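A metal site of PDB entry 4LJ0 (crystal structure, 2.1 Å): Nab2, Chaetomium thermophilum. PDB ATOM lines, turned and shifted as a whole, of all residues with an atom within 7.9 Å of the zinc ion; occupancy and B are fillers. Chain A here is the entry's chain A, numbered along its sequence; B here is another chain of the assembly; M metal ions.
The zinc ion is bound by NE2 of His 60.
The side-chain sulfur (SG) of Cys 51 is bound to the zinc ion (2.2 Å).
The side-chain sulfur (SG) of Cys 56 is bound to the zinc ion (2.3 Å).
SG of Cys 46 binds the zinc ion.
The zinc ion has four donor atoms within binding distance.
ND1 of His 60 is in hydrogen-bond range of OE1 of Glu 31.
N6 of A 4 of chain B sits close to SG of Cys 51 (3.0 Å).
The backbone NH of Asn 53 lies close to the side-chain sulfur of Cys 51 (3.6 Å).
N of Phe 58 sits close to SG of Cys 56 (3.7 Å).
OD1 of Asn 53 sits at hydrogen-bond distance from N of Cys 56 (3.4 Å).
O of Cys 56 lies close to N of Gly 29, 3.4 Å away.
The side-chain sulfur (SG) of Cys 46 sits close to the backbone NH (N) of Phe 48 (3.5 Å).
The backbone NH of Cys 46 sits at hydrogen-bond distance from the backbone carbonyl oxygen of Leu 59, at 2.8 Å.
Of the 23 residues printed, 4 come within 4 Å of the zinc ion.
The nearest printed residue that does not touch the zinc ion is A 4 of chain B (4.01 Å).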
ATOM      1  N   GLY A  29     -28.878 -20.546  10.582  1.00  0.00           N
ATOM      2  CA  GLY A  29     -27.736 -20.034  11.334  1.00  0.00           C
ATOM      3  C   GLY A  29     -26.813 -19.213  10.453  1.00  0.00           C
ATOM      4  O   GLY A  29     -26.926 -19.212   9.227  1.00  0.00           O
ATOM      5  N   GLU A  31     -23.868 -19.837   9.874  1.00  0.00           N
ATOM      6  CA  GLU A  31     -22.964 -20.751   9.168  1.00  0.00           C
ATOM      7  C   GLU A  31     -23.634 -21.434   7.971  1.00  0.00           C
ATOM      8  O   GLU A  31     -23.057 -22.347   7.377  1.00  0.00           O
ATOM      9  CB  GLU A  31     -22.398 -21.805  10.130  1.00  0.00           C
ATOM     10  CG  GLU A  31     -23.367 -22.912  10.553  1.00  0.00           C
ATOM     11  CD  GLU A  31     -24.310 -22.515  11.675  1.00  0.00           C
ATOM     12  OE1 GLU A  31     -24.372 -21.322  12.035  1.00  0.00           O
ATOM     13  OE2 GLU A  31     -24.996 -23.418  12.208  1.00  0.00           O
ATOM     14  N   THR A  44     -22.495 -12.552  14.432  1.00  0.00           N
ATOM     15  CA  THR A  44     -22.404 -12.647  15.886  1.00  0.00           C
ATOM     16  C   THR A  44     -22.441 -14.108  16.318  1.00  0.00           C
ATOM     17  O   THR A  44     -23.397 -14.818  16.013  1.00  0.00           O
ATOM     18  CB  THR A  44     -23.571 -11.902  16.568  1.00  0.00           C
ATOM     19  OG1 THR A  44     -23.556 -10.526  16.167  1.00  0.00           O
ATOM     20  CG2 THR A  44     -23.457 -11.991  18.077  1.00  0.00           C
ATOM     21  N   PRO A  45     -21.389 -14.586  17.020  1.00  0.00           N
ATOM     22  CA  PRO A  45     -21.404 -15.980  17.478  1.00  0.00           C
ATOM     23  C   PRO A  45     -22.520 -16.298  18.465  1.00  0.00           C
ATOM     24  O   PRO A  45     -22.870 -15.470  19.313  1.00  0.00           O
ATOM     25  CB  PRO A  45     -20.025 -16.144  18.150  1.00  0.00           C
ATOM     26  CG  PRO A  45     -19.447 -14.784  18.260  1.00  0.00           C
ATOM     27  CD  PRO A  45     -20.062 -13.954  17.204  1.00  0.00           C
ATOM     28  N   CYS A  46     -23.082 -17.499  18.351  1.00  0.00           N
ATOM     29  CA  CYS A  46     -24.060 -17.989  19.302  1.00  0.00           C
ATOM     30  C   CYS A  46     -23.375 -18.234  20.639  1.00  0.00           C
ATOM     31  O   CYS A  46     -22.257 -18.764  20.679  1.00  0.00           O
ATOM     32  CB  CYS A  46     -24.695 -19.280  18.794  1.00  0.00           C
ATOM     33  SG  CYS A  46     -25.786 -20.089  19.971  1.00  0.00           S
ATOM     34  N   LYS A  47     -24.033 -17.857  21.722  1.00  0.00           N
ATOM     35  CA  LYS A  47     -23.431 -17.907  23.058  1.00  0.00           C
ATOM     36  C   LYS A  47     -23.688 -19.223  23.770  1.00  0.00           C
ATOM     37  O   LYS A  47     -23.084 -19.492  24.805  1.00  0.00           O
ATOM     38  CB  LYS A  47     -23.961 -16.743  23.907  1.00  0.00           C
ATOM     39  CG  LYS A  47     -25.450 -16.827  24.213  1.00  0.00           C
ATOM     40  CD  LYS A  47     -25.943 -15.596  24.963  1.00  0.00           C
ATOM     41  CE  LYS A  47     -27.437 -15.692  25.240  1.00  0.00           C
ATOM     42  NZ  LYS A  47     -27.953 -14.551  26.064  1.00  0.00           N
ATOM     43  N   PHE A  48     -24.562 -20.055  23.218  1.00  0.00           N
ATOM     44  CA  PHE A  48     -24.951 -21.301  23.877  1.00  0.00           C
ATOM     45  C   PHE A  48     -24.042 -22.466  23.492  1.00  0.00           C
ATOM     46  O   PHE A  48     -23.734 -22.660  22.312  1.00  0.00           O
ATOM     47  CB  PHE A  48     -26.397 -21.649  23.544  1.00  0.00           C
ATOM     48  CG  PHE A  48     -27.384 -20.674  24.103  1.00  0.00           C
ATOM     49  CD1 PHE A  48     -27.853 -20.790  25.397  1.00  0.00           C
ATOM     50  CD2 PHE A  48     -27.860 -19.624  23.323  1.00  0.00           C
ATOM     51  CE1 PHE A  48     -28.762 -19.893  25.912  1.00  0.00           C
ATOM     52  CE2 PHE A  48     -28.762 -18.722  23.834  1.00  0.00           C
ATOM     53  CZ  PHE A  48     -29.221 -18.855  25.127  1.00  0.00           C
ATOM     54  N   ARG A  49     -23.613 -23.221  24.495  1.00  0.00           N
ATOM     55  CA  ARG A  49     -22.754 -24.385  24.273  1.00  0.00           C
ATOM     56  C   ARG A  49     -23.211 -25.562  25.114  1.00  0.00           C
ATOM     57  O   ARG A  49     -22.941 -25.610  26.315  1.00  0.00           O
ATOM     58  CB  ARG A  49     -21.300 -24.044  24.613  1.00  0.00           C
ATOM     59  CG  ARG A  49     -20.687 -23.022  23.662  1.00  0.00           C
ATOM     60  CD  ARG A  49     -19.182 -22.975  23.788  1.00  0.00           C
ATOM     61  NE  ARG A  49     -18.598 -22.047  22.816  1.00  0.00           N
ATOM     62  CZ  ARG A  49     -18.280 -22.377  21.562  1.00  0.00           C
ATOM     63  NH1 ARG A  49     -18.483 -23.617  21.121  1.00  0.00           N
ATOM     64  NH2 ARG A  49     -17.760 -21.467  20.748  1.00  0.00           N
ATOM     65  N   PRO A  50     -23.917 -26.524  24.509  1.00  0.00           N
ATOM     66  CA  PRO A  50     -24.345 -26.565  23.102  1.00  0.00           C
ATOM     67  C   PRO A  50     -25.558 -25.685  22.840  1.00  0.00           C
ATOM     68  O   PRO A  50     -26.315 -25.393  23.769  1.00  0.00           O
ATOM     69  CB  PRO A  50     -24.715 -28.028  22.898  1.00  0.00           C
ATOM     70  CG  PRO A  50     -25.177 -28.478  24.230  1.00  0.00           C
ATOM     71  CD  PRO A  50     -24.317 -27.748  25.224  1.00  0.00           C
ATOM     72  N   CYS A  51     -25.746 -25.274  21.584  1.00  0.00           N
ATOM     73  CA  CYS A  51     -26.971 -24.592  21.178  1.00  0.00           C
ATOM     74  C   CYS A  51     -27.973 -25.619  20.691  1.00  0.00           C
ATOM     75  O   CYS A  51     -27.657 -26.429  19.822  1.00  0.00           O
ATOM     76  CB  CYS A  51     -26.681 -23.583  20.066  1.00  0.00           C
ATOM     77  SG  CYS A  51     -28.179 -22.880  19.334  1.00  0.00           S
ATOM     78  N   THR A  52     -29.179 -25.582  21.236  1.00  0.00           N
ATOM     79  CA  THR A  52     -30.222 -26.555  20.891  1.00  0.00           C
ATOM     80  C   THR A  52     -31.446 -25.873  20.277  1.00  0.00           C
ATOM     81  O   THR A  52     -32.502 -26.475  20.164  1.00  0.00           O
ATOM     82  CB  THR A  52     -30.650 -27.367  22.122  1.00  0.00           C
ATOM     83  OG1 THR A  52     -31.133 -26.481  23.137  1.00  0.00           O
ATOM     84  CG2 THR A  52     -29.480 -28.173  22.653  1.00  0.00           C
ATOM     85  N   ASN A  53     -31.290 -24.614  19.886  1.00  0.00           N
ATOM     86  CA  ASN A  53     -32.322 -23.924  19.128  1.00  0.00           C
ATOM     87  C   ASN A  53     -32.078 -24.190  17.646  1.00  0.00           C
ATOM     88  O   ASN A  53     -31.151 -23.641  17.057  1.00  0.00           O
ATOM     89  CB  ASN A  53     -32.289 -22.431  19.434  1.00  0.00           C
ATOM     90  CG  ASN A  53     -33.271 -21.635  18.598  1.00  0.00           C
ATOM     91  OD1 ASN A  53     -34.032 -22.195  17.814  1.00  0.00           O
ATOM     92  ND2 ASN A  53     -33.275 -20.312  18.798  1.00  0.00           N
ATOM     93  N   ARG A  54     -32.914 -25.017  17.023  1.00  0.00           N
ATOM     94  CA  ARG A  54     -32.659 -25.439  15.653  1.00  0.00           C
ATOM     95  C   ARG A  54     -33.044 -24.378  14.606  1.00  0.00           C
ATOM     96  O   ARG A  54     -32.812 -24.579  13.415  1.00  0.00           O
ATOM     97  CB  ARG A  54     -33.324 -26.781  15.360  1.00  0.00           C
ATOM     98  CG  ARG A  54     -32.582 -27.964  15.971  1.00  0.00           C
ATOM     99  CD  ARG A  54     -33.060 -28.294  17.393  1.00  0.00           C
ATOM    100  NE  ARG A  54     -32.107 -29.149  18.095  1.00  0.00           N
ATOM    101  CZ  ARG A  54     -32.348 -29.777  19.239  1.00  0.00           C
ATOM    102  NH1 ARG A  54     -33.538 -29.690  19.826  1.00  0.00           N
ATOM    103  NH2 ARG A  54     -31.403 -30.529  19.790  1.00  0.00           N
ATOM    104  N   SER A  55     -33.590 -23.248  15.063  1.00  0.00           N
ATOM    105  CA  SER A  55     -33.796 -22.084  14.201  1.00  0.00           C
ATOM    106  C   SER A  55     -32.937 -20.904  14.663  1.00  0.00           C
ATOM    107  O   SER A  55     -33.229 -19.744  14.349  1.00  0.00           O
ATOM    108  CB  SER A  55     -35.277 -21.678  14.173  1.00  0.00           C
ATOM    109  OG  SER A  55     -36.018 -22.543  13.331  1.00  0.00           O
ATOM    110  N   CYS A  56     -31.869 -21.192  15.402  1.00  0.00           N
ATOM    111  CA  CYS A  56     -30.970 -20.155  15.897  1.00  0.00           C
ATOM    112  C   CYS A  56     -30.307 -19.426  14.731  1.00  0.00           C
ATOM    113  O   CYS A  56     -29.686 -20.069  13.890  1.00  0.00           O
ATOM    114  CB  CYS A  56     -29.903 -20.772  16.795  1.00  0.00           C
ATOM    115  SG  CYS A  56     -28.809 -19.566  17.592  1.00  0.00           S
ATOM    116  N   PRO A  57     -30.448 -18.093  14.660  1.00  0.00           N
ATOM    117  CA  PRO A  57     -29.883 -17.332  13.542  1.00  0.00           C
ATOM    118  C   PRO A  57     -28.430 -16.944  13.757  1.00  0.00           C
ATOM    119  O   PRO A  57     -27.769 -16.451  12.839  1.00  0.00           O
ATOM    120  CB  PRO A  57     -30.737 -16.068  13.511  1.00  0.00           C
ATOM    121  CG  PRO A  57     -31.114 -15.859  14.935  1.00  0.00           C
ATOM    122  CD  PRO A  57     -31.297 -17.234  15.514  1.00  0.00           C
ATOM    123  N   PHE A  58     -27.909 -17.152  14.961  1.00  0.00           N
ATOM    124  CA  PHE A  58     -26.551 -16.733  15.256  1.00  0.00           C
ATOM    125  C   PHE A  58     -25.528 -17.668  14.612  1.00  0.00           C
ATOM    126  O   PHE A  58     -25.882 -18.662  13.986  1.00  0.00           O
ATOM    127  CB  PHE A  58     -26.373 -16.614  16.767  1.00  0.00           C
ATOM    128  CG  PHE A  58     -27.149 -15.479  17.362  1.00  0.00           C
ATOM    129  CD1 PHE A  58     -28.443 -15.678  17.819  1.00  0.00           C
ATOM    130  CD2 PHE A  58     -26.599 -14.211  17.428  1.00  0.00           C
ATOM    131  CE1 PHE A  58     -29.165 -14.620  18.346  1.00  0.00           C
ATOM    132  CE2 PHE A  58     -27.318 -13.152  17.965  1.00  0.00           C
ATOM    133  CZ  PHE A  58     -28.607 -13.360  18.421  1.00  0.00           C
ATOM    134  N   LEU A  59     -24.259 -17.304  14.732  1.00  0.00           N
ATOM    135  CA  LEU A  59     -23.181 -18.007  14.048  1.00  0.00           C
ATOM    136  C   LEU A  59     -22.617 -19.112  14.941  1.00  0.00           C
ATOM    137  O   LEU A  59     -22.192 -18.848  16.072  1.00  0.00           O
ATOM    138  CB  LEU A  59     -22.082 -17.006  13.682  1.00  0.00           C
ATOM    139  CG  LEU A  59     -20.819 -17.524  12.987  1.00  0.00           C
ATOM    140  CD1 LEU A  59     -21.151 -18.077  11.603  1.00  0.00           C
ATOM    141  CD2 LEU A  59     -19.780 -16.423  12.884  1.00  0.00           C
ATOM    142  N   HIS A  60     -22.611 -20.332  14.433  1.00  0.00           N
ATOM    143  CA  HIS A  60     -22.141 -21.487  15.196  1.00  0.00           C
ATOM    144  C   HIS A  60     -20.837 -22.053  14.631  1.00  0.00           C
ATOM    145  O   HIS A  60     -20.585 -21.966  13.429  1.00  0.00           O
ATOM    146  CB  HIS A  60     -23.207 -22.578  15.179  1.00  0.00           C
ATOM    147  CG  HIS A  60     -24.534 -22.122  15.690  1.00  0.00           C
ATOM    148  ND1 HIS A  60     -25.479 -21.527  14.885  1.00  0.00           N
ATOM    149  CD2 HIS A  60     -25.059 -22.138  16.941  1.00  0.00           C
ATOM    150  CE1 HIS A  60     -26.540 -21.211  15.609  1.00  0.00           C
ATOM    151  NE2 HIS A  60     -26.307 -21.573  16.863  1.00  0.00           N
ATOM    152  N   GLN A  64     -20.725 -27.059  17.825  1.00  0.00           N
ATOM    153  CA  GLN A  64     -21.439 -26.229  18.789  1.00  0.00           C
ATOM    154  C   GLN A  64     -22.923 -26.585  18.865  1.00  0.00           C
ATOM    155  O   GLN A  64     -23.568 -26.379  19.889  1.00  0.00           O
ATOM    156  CB  GLN A  64     -21.270 -24.752  18.465  1.00  0.00           C
ATOM    157  CG  GLN A  64     -21.964 -23.832  19.454  1.00  0.00           C
ATOM    158  CD  GLN A  64     -21.597 -22.375  19.279  1.00  0.00           C
ATOM    159  OE1 GLN A  64     -20.896 -22.007  18.338  1.00  0.00           O
ATOM    160  NE2 GLN A  64     -22.073 -21.531  20.177  1.00  0.00           N
ATOM    161  N   ARG A  65     -23.461 -27.113  17.769  1.00  0.00           N
ATOM    162  CA  ARG A  65     -24.859 -27.522  17.718  1.00  0.00           C
ATOM    163  C   ARG A  65     -25.059 -28.773  18.550  1.00  0.00           C
ATOM    164  O   ARG A  65     -24.220 -29.672  18.543  1.00  0.00           O
ATOM    165  CB  ARG A  65     -25.280 -27.786  16.280  1.00  0.00           C
ATOM    166  CG  ARG A  65     -25.243 -26.573  15.378  1.00  0.00           C
ATOM    167  CD  ARG A  65     -26.509 -25.751  15.483  1.00  0.00           C
ATOM    168  NE  ARG A  65     -26.665 -24.883  14.321  1.00  0.00           N
ATOM    169  CZ  ARG A  65     -27.780 -24.219  14.013  1.00  0.00           C
ATOM    170  NH1 ARG A  65     -28.859 -24.332  14.786  1.00  0.00           N
ATOM    171  NH2 ARG A  65     -27.818 -23.455  12.936  1.00  0.00           N
ATOM    172  P     A B   3     -34.848 -11.939  25.174  1.00  0.00           P
ATOM    173  OP1   A B   3     -35.720 -13.134  25.111  1.00  0.00           O
ATOM    174  OP2   A B   3     -34.154 -11.608  26.448  1.00  0.00           O
ATOM    175  O5'   A B   3     -33.718 -12.081  24.052  1.00  0.00           O
ATOM    176  C5'   A B   3     -34.001 -12.726  22.811  1.00  0.00           C
ATOM    177  C4'   A B   3     -33.504 -14.160  22.781  1.00  0.00           C
ATOM    178  O4'   A B   3     -32.301 -14.239  21.970  1.00  0.00           O
ATOM    179  C3'   A B   3     -33.153 -14.779  24.136  1.00  0.00           C
ATOM    180  O3'   A B   3     -33.612 -16.137  24.196  1.00  0.00           O
ATOM    181  C2'   A B   3     -31.627 -14.744  24.159  1.00  0.00           C
ATOM    182  O2'   A B   3     -31.027 -15.718  24.977  1.00  0.00           O
ATOM    183  C1'   A B   3     -31.302 -14.954  22.680  1.00  0.00           C
ATOM    184  N9    A B   3     -29.965 -14.474  22.301  1.00  0.00           N
ATOM    185  C8    A B   3     -29.432 -13.209  22.408  1.00  0.00           C
ATOM    186  N7    A B   3     -28.191 -13.136  21.998  1.00  0.00           N
ATOM    187  C5    A B   3     -27.874 -14.423  21.599  1.00  0.00           C
ATOM    188  C6    A B   3     -26.707 -15.012  21.061  1.00  0.00           C
ATOM    189  N6    A B   3     -25.577 -14.353  20.822  1.00  0.00           N
ATOM    190  N1    A B   3     -26.746 -16.338  20.770  1.00  0.00           N
ATOM    191  C2    A B   3     -27.871 -17.006  21.009  1.00  0.00           C
ATOM    192  N3    A B   3     -29.028 -16.568  21.507  1.00  0.00           N
ATOM    193  C4    A B   3     -28.967 -15.251  21.779  1.00  0.00           C
ATOM    194  P     A B   4     -34.621 -16.610  25.364  1.00  0.00           P
ATOM    195  OP1   A B   4     -35.758 -17.303  24.707  1.00  0.00           O
ATOM    196  OP2   A B   4     -34.883 -15.489  26.293  1.00  0.00           O
ATOM    197  O5'   A B   4     -33.782 -17.691  26.173  1.00  0.00           O
ATOM    198  C5'   A B   4     -34.191 -18.075  27.486  1.00  0.00           C
ATOM    199  C4'   A B   4     -33.550 -19.363  27.912  1.00  0.00           C
ATOM    200  O4'   A B   4     -33.802 -20.398  26.922  1.00  0.00           O
ATOM    201  C3'   A B   4     -32.035 -19.346  28.049  1.00  0.00           C
ATOM    202  O3'   A B   4     -31.588 -18.792  29.278  1.00  0.00           O
ATOM    203  C2'   A B   4     -31.675 -20.817  27.873  1.00  0.00           C
ATOM    204  O2'   A B   4     -31.911 -21.563  29.061  1.00  0.00           O
ATOM    205  C1'   A B   4     -32.681 -21.242  26.804  1.00  0.00           C
ATOM    206  N9    A B   4     -32.126 -21.106  25.450  1.00  0.00           N
ATOM    207  C8    A B   4     -32.336 -20.079  24.563  1.00  0.00           C
ATOM    208  N7    A B   4     -31.701 -20.220  23.417  1.00  0.00           N
ATOM    209  C5    A B   4     -31.035 -21.430  23.573  1.00  0.00           C
ATOM    210  C6    A B   4     -30.186 -22.150  22.713  1.00  0.00           C
ATOM    211  N6    A B   4     -29.859 -21.730  21.484  1.00  0.00           N
ATOM    212  N1    A B   4     -29.683 -23.322  23.160  1.00  0.00           N
ATOM    213  C2    A B   4     -30.010 -23.732  24.399  1.00  0.00           C
ATOM    214  N3    A B   4     -30.800 -23.144  25.294  1.00  0.00           N
ATOM    215  C4    A B   4     -31.281 -21.991  24.819  1.00  0.00           C
HETATM  216 ZN    ZN M   1     -27.312 -21.022  18.470  1.00  0.00          ZN
